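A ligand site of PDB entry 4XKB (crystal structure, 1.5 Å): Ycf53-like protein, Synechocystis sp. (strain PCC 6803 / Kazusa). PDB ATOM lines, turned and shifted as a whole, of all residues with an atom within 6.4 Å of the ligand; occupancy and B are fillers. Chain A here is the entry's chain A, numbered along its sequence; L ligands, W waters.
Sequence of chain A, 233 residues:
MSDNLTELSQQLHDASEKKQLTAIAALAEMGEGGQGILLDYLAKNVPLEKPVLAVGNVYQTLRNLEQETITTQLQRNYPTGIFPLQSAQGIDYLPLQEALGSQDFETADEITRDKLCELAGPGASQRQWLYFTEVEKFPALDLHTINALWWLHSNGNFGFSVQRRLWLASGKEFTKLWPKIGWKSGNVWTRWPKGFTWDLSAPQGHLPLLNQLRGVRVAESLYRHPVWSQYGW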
ATOM      1  N   ASP A 109     -25.353  -5.872  -0.091  1.00  0.00           N
ATOM      2  CA  ASP A 109     -24.305  -6.585   0.613  1.00  0.00           C
ATOM      3  C   ASP A 109     -23.333  -5.600   1.285  1.00  0.00           C
ATOM      4  O   ASP A 109     -22.967  -5.779   2.441  1.00  0.00           O
ATOM      5  CB  ASP A 109     -23.556  -7.502  -0.355  1.00  0.00           C
ATOM      6  CG  ASP A 109     -22.620  -8.433   0.359  1.00  0.00           C
ATOM      7  OD1 ASP A 109     -23.101  -9.211   1.199  1.00  0.00           O
ATOM      8  OD2 ASP A 109     -21.402  -8.385   0.083  1.00  0.00           O
ATOM      9  N   ARG A 113     -22.770  -5.111   5.410  1.00  0.00           N
ATOM     10  CA  ARG A 113     -21.448  -5.177   6.032  1.00  0.00           C
ATOM     11  C   ARG A 113     -21.195  -3.945   6.898  1.00  0.00           C
ATOM     12  O   ARG A 113     -20.746  -4.047   8.049  1.00  0.00           O
ATOM     13  CB  ARG A 113     -20.389  -5.307   4.940  1.00  0.00           C
ATOM     14  CG  ARG A 113     -18.953  -5.345   5.425  1.00  0.00           C
ATOM     15  CD  ARG A 113     -18.023  -5.992   4.389  1.00  0.00           C
ATOM     16  NE  ARG A 113     -18.095  -5.360   3.077  1.00  0.00           N
ATOM     17  CZ  ARG A 113     -18.742  -5.857   2.017  1.00  0.00           C
ATOM     18  NH1 ARG A 113     -19.398  -7.000   2.114  1.00  0.00           N
ATOM     19  NH2 ARG A 113     -18.739  -5.204   0.860  1.00  0.00           N
ATOM     20  N   GLN A 128     -13.364  -1.471  10.732  1.00  0.00           N
ATOM     21  CA  GLN A 128     -14.161  -1.934   9.586  1.00  0.00           C
ATOM     22  C   GLN A 128     -14.172  -3.461   9.432  1.00  0.00           C
ATOM     23  O   GLN A 128     -14.234  -3.989   8.314  1.00  0.00           O
ATOM     24  CB  GLN A 128     -13.795  -1.223   8.282  1.00  0.00           C
ATOM     25  CG  GLN A 128     -14.340   0.215   8.182  1.00  0.00           C
ATOM     26  CD  GLN A 128     -15.864   0.272   8.045  1.00  0.00           C
ATOM     27  OE1 GLN A 128     -16.412   0.026   6.968  1.00  0.00           O
ATOM     28  NE2 GLN A 128     -16.542   0.609   9.134  1.00  0.00           N
ATOM     29  N   TRP A 129     -14.145  -4.136  10.562  1.00  0.00           N
ATOM     30  CA  TRP A 129     -14.369  -5.582  10.614  1.00  0.00           C
ATOM     31  C   TRP A 129     -14.709  -5.963  12.039  1.00  0.00           C
ATOM     32  O   TRP A 129     -14.485  -5.182  12.954  1.00  0.00           O
ATOM     33  CB  TRP A 129     -13.175  -6.389  10.074  1.00  0.00           C
ATOM     34  CG  TRP A 129     -11.810  -5.967  10.549  1.00  0.00           C
ATOM     35  CD1 TRP A 129     -11.012  -4.987   9.997  1.00  0.00           C
ATOM     36  CD2 TRP A 129     -11.062  -6.529  11.628  1.00  0.00           C
ATOM     37  NE1 TRP A 129      -9.831  -4.901  10.690  1.00  0.00           N
ATOM     38  CE2 TRP A 129      -9.833  -5.843  11.688  1.00  0.00           C
ATOM     39  CE3 TRP A 129     -11.314  -7.554  12.554  1.00  0.00           C
ATOM     40  CZ2 TRP A 129      -8.851  -6.137  12.645  1.00  0.00           C
ATOM     41  CZ3 TRP A 129     -10.331  -7.844  13.497  1.00  0.00           C
ATOM     42  CH2 TRP A 129      -9.115  -7.137  13.532  1.00  0.00           C
ATOM     43  N   TRP A 183     -19.255 -20.165  -2.170  1.00  0.00           N
ATOM     44  CA  TRP A 183     -18.125 -19.354  -1.694  1.00  0.00           C
ATOM     45  C   TRP A 183     -16.783 -20.018  -1.936  1.00  0.00           C
ATOM     46  O   TRP A 183     -15.727 -19.391  -1.807  1.00  0.00           O
ATOM     47  CB  TRP A 183     -18.266 -18.994  -0.217  1.00  0.00           C
ATOM     48  CG  TRP A 183     -19.438 -18.115   0.095  1.00  0.00           C
ATOM     49  CD1 TRP A 183     -20.388 -17.658  -0.785  1.00  0.00           C
ATOM     50  CD2 TRP A 183     -19.795 -17.588   1.372  1.00  0.00           C
ATOM     51  NE1 TRP A 183     -21.305 -16.875  -0.122  1.00  0.00           N
ATOM     52  CE2 TRP A 183     -20.968 -16.822   1.201  1.00  0.00           C
ATOM     53  CE3 TRP A 183     -19.239 -17.688   2.660  1.00  0.00           C
ATOM     54  CZ2 TRP A 183     -21.600 -16.168   2.261  1.00  0.00           C
ATOM     55  CZ3 TRP A 183     -19.867 -17.060   3.705  1.00  0.00           C
ATOM     56  CH2 TRP A 183     -21.038 -16.302   3.502  1.00  0.00           C
ATOM     57  N   TRP A 189     -11.229 -20.471  -3.451  1.00  0.00           N
ATOM     58  CA  TRP A 189     -12.178 -19.533  -2.853  1.00  0.00           C
ATOM     59  C   TRP A 189     -12.728 -18.593  -3.921  1.00  0.00           C
ATOM     60  O   TRP A 189     -11.988 -18.133  -4.799  1.00  0.00           O
ATOM     61  CB  TRP A 189     -11.523 -18.696  -1.759  1.00  0.00           C
ATOM     62  CG  TRP A 189     -11.273 -19.438  -0.479  1.00  0.00           C
ATOM     63  CD1 TRP A 189     -10.108 -20.036  -0.093  1.00  0.00           C
ATOM     64  CD2 TRP A 189     -12.210 -19.657   0.574  1.00  0.00           C
ATOM     65  NE1 TRP A 189     -10.268 -20.613   1.147  1.00  0.00           N
ATOM     66  CE2 TRP A 189     -11.549 -20.403   1.573  1.00  0.00           C
ATOM     67  CE3 TRP A 189     -13.551 -19.302   0.778  1.00  0.00           C
ATOM     68  CZ2 TRP A 189     -12.182 -20.778   2.763  1.00  0.00           C
ATOM     69  CZ3 TRP A 189     -14.175 -19.696   1.948  1.00  0.00           C
ATOM     70  CH2 TRP A 189     -13.495 -20.428   2.923  1.00  0.00           C
ATOM     71  N   THR A 190     -14.018 -18.314  -3.847  1.00  0.00           N
ATOM     72  CA  THR A 190     -14.613 -17.318  -4.724  1.00  0.00           C
ATOM     73  C   THR A 190     -13.983 -15.966  -4.430  1.00  0.00           C
ATOM     74  O   THR A 190     -13.835 -15.580  -3.275  1.00  0.00           O
ATOM     75  CB  THR A 190     -16.129 -17.313  -4.527  1.00  0.00           C
ATOM     76  OG1 THR A 190     -16.626 -18.640  -4.725  1.00  0.00           O
ATOM     77  CG2 THR A 190     -16.809 -16.346  -5.495  1.00  0.00           C
ATOM     78  N   TRP A 192     -13.579 -11.990  -4.279  1.00  0.00           N
ATOM     79  CA  TRP A 192     -14.391 -10.787  -4.129  1.00  0.00           C
ATOM     80  C   TRP A 192     -13.747  -9.637  -4.895  1.00  0.00           C
ATOM     81  O   TRP A 192     -12.539  -9.466  -4.835  1.00  0.00           O
ATOM     82  CB  TRP A 192     -14.487 -10.433  -2.657  1.00  0.00           C
ATOM     83  CG  TRP A 192     -15.346  -9.247  -2.390  1.00  0.00           C
ATOM     84  CD1 TRP A 192     -16.702  -9.245  -2.201  1.00  0.00           C
ATOM     85  CD2 TRP A 192     -14.922  -7.885  -2.277  1.00  0.00           C
ATOM     86  NE1 TRP A 192     -17.146  -7.968  -1.976  1.00  0.00           N
ATOM     87  CE2 TRP A 192     -16.072  -7.118  -2.014  1.00  0.00           C
ATOM     88  CE3 TRP A 192     -13.685  -7.243  -2.364  1.00  0.00           C
ATOM     89  CZ2 TRP A 192     -16.017  -5.736  -1.849  1.00  0.00           C
ATOM     90  CZ3 TRP A 192     -13.634  -5.869  -2.195  1.00  0.00           C
ATOM     91  CH2 TRP A 192     -14.798  -5.136  -1.936  1.00  0.00           C
ATOM     92  N   PHE A 196     -18.432 -13.341  -7.343  1.00  0.00           N
ATOM     93  CA  PHE A 196     -19.724 -13.632  -6.734  1.00  0.00           C
ATOM     94  C   PHE A 196     -20.878 -13.349  -7.696  1.00  0.00           C
ATOM     95  O   PHE A 196     -20.702 -12.660  -8.698  1.00  0.00           O
ATOM     96  CB  PHE A 196     -19.877 -12.855  -5.425  1.00  0.00           C
ATOM     97  CG  PHE A 196     -18.956 -13.351  -4.360  1.00  0.00           C
ATOM     98  CD1 PHE A 196     -19.328 -14.430  -3.559  1.00  0.00           C
ATOM     99  CD2 PHE A 196     -17.701 -12.799  -4.206  1.00  0.00           C
ATOM    100  CE1 PHE A 196     -18.473 -14.925  -2.605  1.00  0.00           C
ATOM    101  CE2 PHE A 196     -16.834 -13.281  -3.238  1.00  0.00           C
ATOM    102  CZ  PHE A 196     -17.222 -14.347  -2.435  1.00  0.00           C
ATOM    103  N   TRP A 198     -24.364 -11.681  -8.099  1.00  0.00           N
ATOM    104  CA  TRP A 198     -25.128 -10.622  -7.460  1.00  0.00           C
ATOM    105  C   TRP A 198     -26.569 -10.592  -7.941  1.00  0.00           C
ATOM    106  O   TRP A 198     -27.149  -9.509  -8.103  1.00  0.00           O
ATOM    107  CB  TRP A 198     -24.445  -9.285  -7.695  1.00  0.00           C
ATOM    108  CG  TRP A 198     -23.038  -9.262  -7.208  1.00  0.00           C
ATOM    109  CD1 TRP A 198     -21.904  -9.255  -7.959  1.00  0.00           C
ATOM    110  CD2 TRP A 198     -22.621  -9.245  -5.837  1.00  0.00           C
ATOM    111  NE1 TRP A 198     -20.794  -9.235  -7.145  1.00  0.00           N
ATOM    112  CE2 TRP A 198     -21.204  -9.220  -5.833  1.00  0.00           C
ATOM    113  CE3 TRP A 198     -23.296  -9.247  -4.616  1.00  0.00           C
ATOM    114  CZ2 TRP A 198     -20.460  -9.202  -4.653  1.00  0.00           C
ATOM    115  CZ3 TRP A 198     -22.554  -9.215  -3.439  1.00  0.00           C
ATOM    116  CH2 TRP A 198     -21.160  -9.197  -3.469  1.00  0.00           C
ATOM    117  N   HIS A 206     -26.340 -17.685  -0.904  1.00  0.00           N
ATOM    118  CA  HIS A 206     -25.144 -17.048  -1.451  1.00  0.00           C
ATOM    119  C   HIS A 206     -24.824 -15.709  -0.775  1.00  0.00           C
ATOM    120  O   HIS A 206     -23.654 -15.373  -0.600  1.00  0.00           O
ATOM    121  CB  HIS A 206     -25.323 -16.806  -2.955  1.00  0.00           C
ATOM    122  CG  HIS A 206     -24.062 -16.434  -3.683  1.00  0.00           C
ATOM    123  ND1 HIS A 206     -22.974 -17.262  -3.786  1.00  0.00           N
ATOM    124  CD2 HIS A 206     -23.771 -15.338  -4.434  1.00  0.00           C
ATOM    125  CE1 HIS A 206     -22.044 -16.688  -4.542  1.00  0.00           C
ATOM    126  NE2 HIS A 206     -22.507 -15.522  -4.942  1.00  0.00           N
ATOM    127  N   LEU A 209     -22.597 -11.841   2.118  1.00  0.00           N
ATOM    128  CA  LEU A 209     -21.251 -12.420   2.253  1.00  0.00           C
ATOM    129  C   LEU A 209     -20.650 -12.210   3.629  1.00  0.00           C
ATOM    130  O   LEU A 209     -20.832 -11.162   4.261  1.00  0.00           O
ATOM    131  CB  LEU A 209     -20.328 -11.816   1.193  1.00  0.00           C
ATOM    132  CG  LEU A 209     -20.744 -11.999  -0.267  1.00  0.00           C
ATOM    133  CD1 LEU A 209     -19.674 -11.428  -1.182  1.00  0.00           C
ATOM    134  CD2 LEU A 209     -20.975 -13.476  -0.554  1.00  0.00           C
ATOM    135  N   LEU A 210     -19.907 -13.215   4.084  1.00  0.00           N
ATOM    136  CA  LEU A 210     -19.100 -13.120   5.302  1.00  0.00           C
ATOM    137  C   LEU A 210     -17.663 -13.451   4.936  1.00  0.00           C
ATOM    138  O   LEU A 210     -17.296 -14.619   4.738  1.00  0.00           O
ATOM    139  CB  LEU A 210     -19.610 -14.082   6.379  1.00  0.00           C
ATOM    140  CG  LEU A 210     -21.018 -13.786   6.871  1.00  0.00           C
ATOM    141  CD1 LEU A 210     -21.599 -14.983   7.629  1.00  0.00           C
ATOM    142  CD2 LEU A 210     -21.032 -12.528   7.757  1.00  0.00           C
ATOM    143  N   ASN A 211     -16.839 -12.417   4.821  1.00  0.00           N
ATOM    144  CA  ASN A 211     -15.441 -12.597   4.439  1.00  0.00           C
ATOM    145  C   ASN A 211     -14.742 -13.595   5.354  1.00  0.00           C
ATOM    146  O   ASN A 211     -14.857 -13.503   6.563  1.00  0.00           O
ATOM    147  CB  ASN A 211     -14.748 -11.236   4.510  1.00  0.00           C
ATOM    148  CG  ASN A 211     -13.321 -11.267   3.984  1.00  0.00           C
ATOM    149  OD1 ASN A 211     -12.797 -12.276   3.517  1.00  0.00           O
ATOM    150  ND2 ASN A 211     -12.688 -10.102   4.047  1.00  0.00           N
ATOM    151  N   GLN A 212     -14.021 -14.553   4.765  1.00  0.00           N
ATOM    152  CA  GLN A 212     -13.331 -15.589   5.549  1.00  0.00           C
ATOM    153  C   GLN A 212     -11.846 -15.280   5.776  1.00  0.00           C
ATOM    154  O   GLN A 212     -11.127 -16.087   6.352  1.00  0.00           O
ATOM    155  CB  GLN A 212     -13.523 -16.961   4.890  1.00  0.00           C
ATOM    156  CG  GLN A 212     -14.963 -17.418   4.971  1.00  0.00           C
ATOM    157  CD  GLN A 212     -15.432 -17.469   6.398  1.00  0.00           C
ATOM    158  OE1 GLN A 212     -14.853 -18.191   7.218  1.00  0.00           O
ATOM    159  NE2 GLN A 212     -16.442 -16.681   6.734  1.00  0.00           N
ATOM    160  N   LEU A 213     -11.433 -14.086   5.373  1.00  0.00           N
ATOM    161  CA  LEU A 213     -10.052 -13.639   5.559  1.00  0.00           C
ATOM    162  C   LEU A 213      -9.571 -13.769   7.002  1.00  0.00           C
ATOM    163  O   LEU A 213      -8.409 -14.060   7.246  1.00  0.00           O
ATOM    164  CB  LEU A 213      -9.928 -12.186   5.112  1.00  0.00           C
ATOM    165  CG  LEU A 213      -8.602 -11.483   5.411  1.00  0.00           C
ATOM    166  CD1 LEU A 213      -7.445 -12.172   4.696  1.00  0.00           C
ATOM    167  CD2 LEU A 213      -8.735 -10.026   5.000  1.00  0.00           C
ATOM    168  N   ARG A 214     -10.463 -13.560   7.963  1.00  0.00           N
ATOM    169  CA  ARG A 214     -10.082 -13.699   9.371  1.00  0.00           C
ATOM    170  C   ARG A 214     -10.722 -14.922  10.026  1.00  0.00           C
ATOM    171  O   ARG A 214     -10.953 -14.933  11.228  1.00  0.00           O
ATOM    172  CB  ARG A 214     -10.401 -12.410  10.155  1.00  0.00           C
ATOM    173  CG  ARG A 214      -9.557 -11.217   9.689  1.00  0.00           C
ATOM    174  CD  ARG A 214     -10.129  -9.876  10.182  1.00  0.00           C
ATOM    175  NE  ARG A 214     -11.447  -9.644   9.591  1.00  0.00           N
ATOM    176  CZ  ARG A 214     -11.673  -9.028   8.437  1.00  0.00           C
ATOM    177  NH1 ARG A 214     -10.658  -8.522   7.750  1.00  0.00           N
ATOM    178  NH2 ARG A 214     -12.909  -8.898   7.986  1.00  0.00           N
HETATM  179  C1  LIG L   1     -12.087  -8.830   0.955  1.00  0.00           C
HETATM  180  C2  LIG L   1     -15.956 -12.112   0.833  1.00  0.00           C
HETATM  181  C3  LIG L   1     -12.697 -15.931   1.371  1.00  0.00           C
HETATM  182  C4  LIG L   1      -8.837 -12.687   1.272  1.00  0.00           C
HETATM  183  N1  LIG L   1     -13.754 -10.776   0.843  1.00  0.00           N
HETATM  184  C5  LIG L   1     -13.434  -9.470   0.972  1.00  0.00           C
HETATM  185  C6  LIG L   1     -14.601  -8.738   1.119  1.00  0.00           C
HETATM  186  C7  LIG L   1     -15.657  -9.653   1.093  1.00  0.00           C
HETATM  187  C8  LIG L   1     -15.101 -10.906   0.916  1.00  0.00           C
HETATM  188  C9  LIG L   1     -17.114  -9.370   1.211  1.00  0.00           C
HETATM  189  C10 LIG L   1     -14.766  -7.264   1.284  1.00  0.00           C
HETATM  190  C11 LIG L   1     -14.875  -6.746   2.679  1.00  0.00           C
HETATM  191  C12 LIG L   1     -13.613  -6.852   3.454  1.00  0.00           C
HETATM  192  O1  LIG L   1     -13.580  -7.494   4.535  1.00  0.00           O
HETATM  193  O2  LIG L   1     -12.578  -6.282   3.019  1.00  0.00           O
HETATM  194  N2  LIG L   1     -14.015 -13.746   1.082  1.00  0.00           N
HETATM  195  C13 LIG L   1     -15.324 -13.446   0.996  1.00  0.00           C
HETATM  196  C14 LIG L   1     -16.084 -14.607   1.086  1.00  0.00           C
HETATM  197  C15 LIG L   1     -15.175 -15.651   1.225  1.00  0.00           C
HETATM  198  C16 LIG L   1     -13.907 -15.086   1.222  1.00  0.00           C
HETATM  199  C17 LIG L   1     -17.572 -14.719   1.040  1.00  0.00           C
HETATM  200  N3  LIG L   1     -11.008 -14.032   1.173  1.00  0.00           N
HETATM  201  C18 LIG L   1     -11.373 -15.268   1.515  1.00  0.00           C
HETATM  202  C19 LIG L   1     -10.294 -15.926   2.061  1.00  0.00           C
HETATM  203  C20 LIG L   1      -9.235 -15.032   2.036  1.00  0.00           C
HETATM  204  C21 LIG L   1      -9.709 -13.867   1.471  1.00  0.00           C
HETATM  205  C22 LIG L   1     -10.260 -17.316   2.580  1.00  0.00           C
HETATM  206  N4  LIG L   1     -10.763 -11.033   1.113  1.00  0.00           N
HETATM  207  C23 LIG L   1      -9.454 -11.350   1.193  1.00  0.00           C
HETATM  208  C24 LIG L   1      -8.691 -10.179   1.167  1.00  0.00           C
HETATM  209  C25 LIG L   1      -9.600  -9.144   1.076  1.00  0.00           C
HETATM  210  C26 LIG L   1     -10.873  -9.696   1.054  1.00  0.00           C
HETATM  211  C27 LIG L   1      -7.203 -10.038   1.237  1.00  0.00           C
HETATM  212  C28 LIG L   1      -9.268  -7.695   1.058  1.00  0.00           C
HETATM  213  C29 LIG L   1      -9.447  -7.093   2.406  1.00  0.00           C
HETATM  214  C30 LIG L   1      -8.775  -5.810   2.742  1.00  0.00           C
HETATM  215  O3  LIG L   1      -7.995  -5.305   1.912  1.00  0.00           O
HETATM  216  O4  LIG L   1      -8.991  -5.248   3.858  1.00  0.00           O
HETATM  217  O   HOH W   1     -11.406  -6.622   5.588  1.00  0.00           O
HETATM  218  O   HOH W   2     -12.636 -13.441  -1.606  1.00  0.00           O
HETATM  219  O   HOH W   3      -8.915  -2.685   3.853  1.00  0.00           O
HETATM  220  O   HOH W   4      -5.623  -6.448   0.704  1.00  0.00           O
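The guanidinium group (NH2) of Arg 214 lies within salt-bridge range of an oxygen (O1) of the ligand, at 3.8 Å.
O1 of the ligand is in hydrogen-bond range of ND2 of Asn 211.
NH1 of Arg 113 lies within salt-bridge range of OD2 of Asp 109 (3.2 Å).
The backbone NH of Leu 209 lies within hydrogen-bond range of the side-chain carboxylate of Asp 109.
O of His 206 sits at hydrogen-bond distance from NE1 of Trp 183 (2.8 Å).
The side-chain amide nitrogen of Gln 212 sits at hydrogen-bond distance from the backbone carbonyl oxygen of Leu 210 (3.0 Å).
O of Trp 183 lies within hydrogen-bond range of N of Thr 190 (2.9 Å).
The side-chain amide oxygen (OD1) of Asn 211 sits at hydrogen-bond distance from the backbone NH (N) of Leu 213, at 2.9 Å.
Arg 113 touches the ligand (NH1 to C9, 3.4 Å).
Trp 183 touches the ligand (CD2 to C17, 3.6 Å).
Trp 189 touches the ligand (CE2 to C22, 3.5 Å).
CD1 of Trp 192 touches C9 of the ligand, at 3.4 Å.
Phe 196 touches the ligand.
Leu 209 touches the ligand (CD2 to C17, 3.96 Å).
Leu 210 touches the ligand (O to C17, 3.7 Å).
Gln 212 touches the ligand (N to C16, 3.6 Å).
CD1 of Leu 213 touches C4 of the ligand, at 3.7 Å.
Hydrophobic or aromatic side chains that line the ligand: Trp 183, Trp 189, Trp 192, Phe 196, Leu 209 and Leu 213.
Water W1 bridges O1 of the ligand (2.6 Å) and NH1 of Arg 214 (3.0 Å).
Water W2 lies within hydrogen-bond range of the backbone carbonyl oxygen (O) of Thr 190, a nitrogen (N2) of the ligand and the backbone NH (N) of Trp 192.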
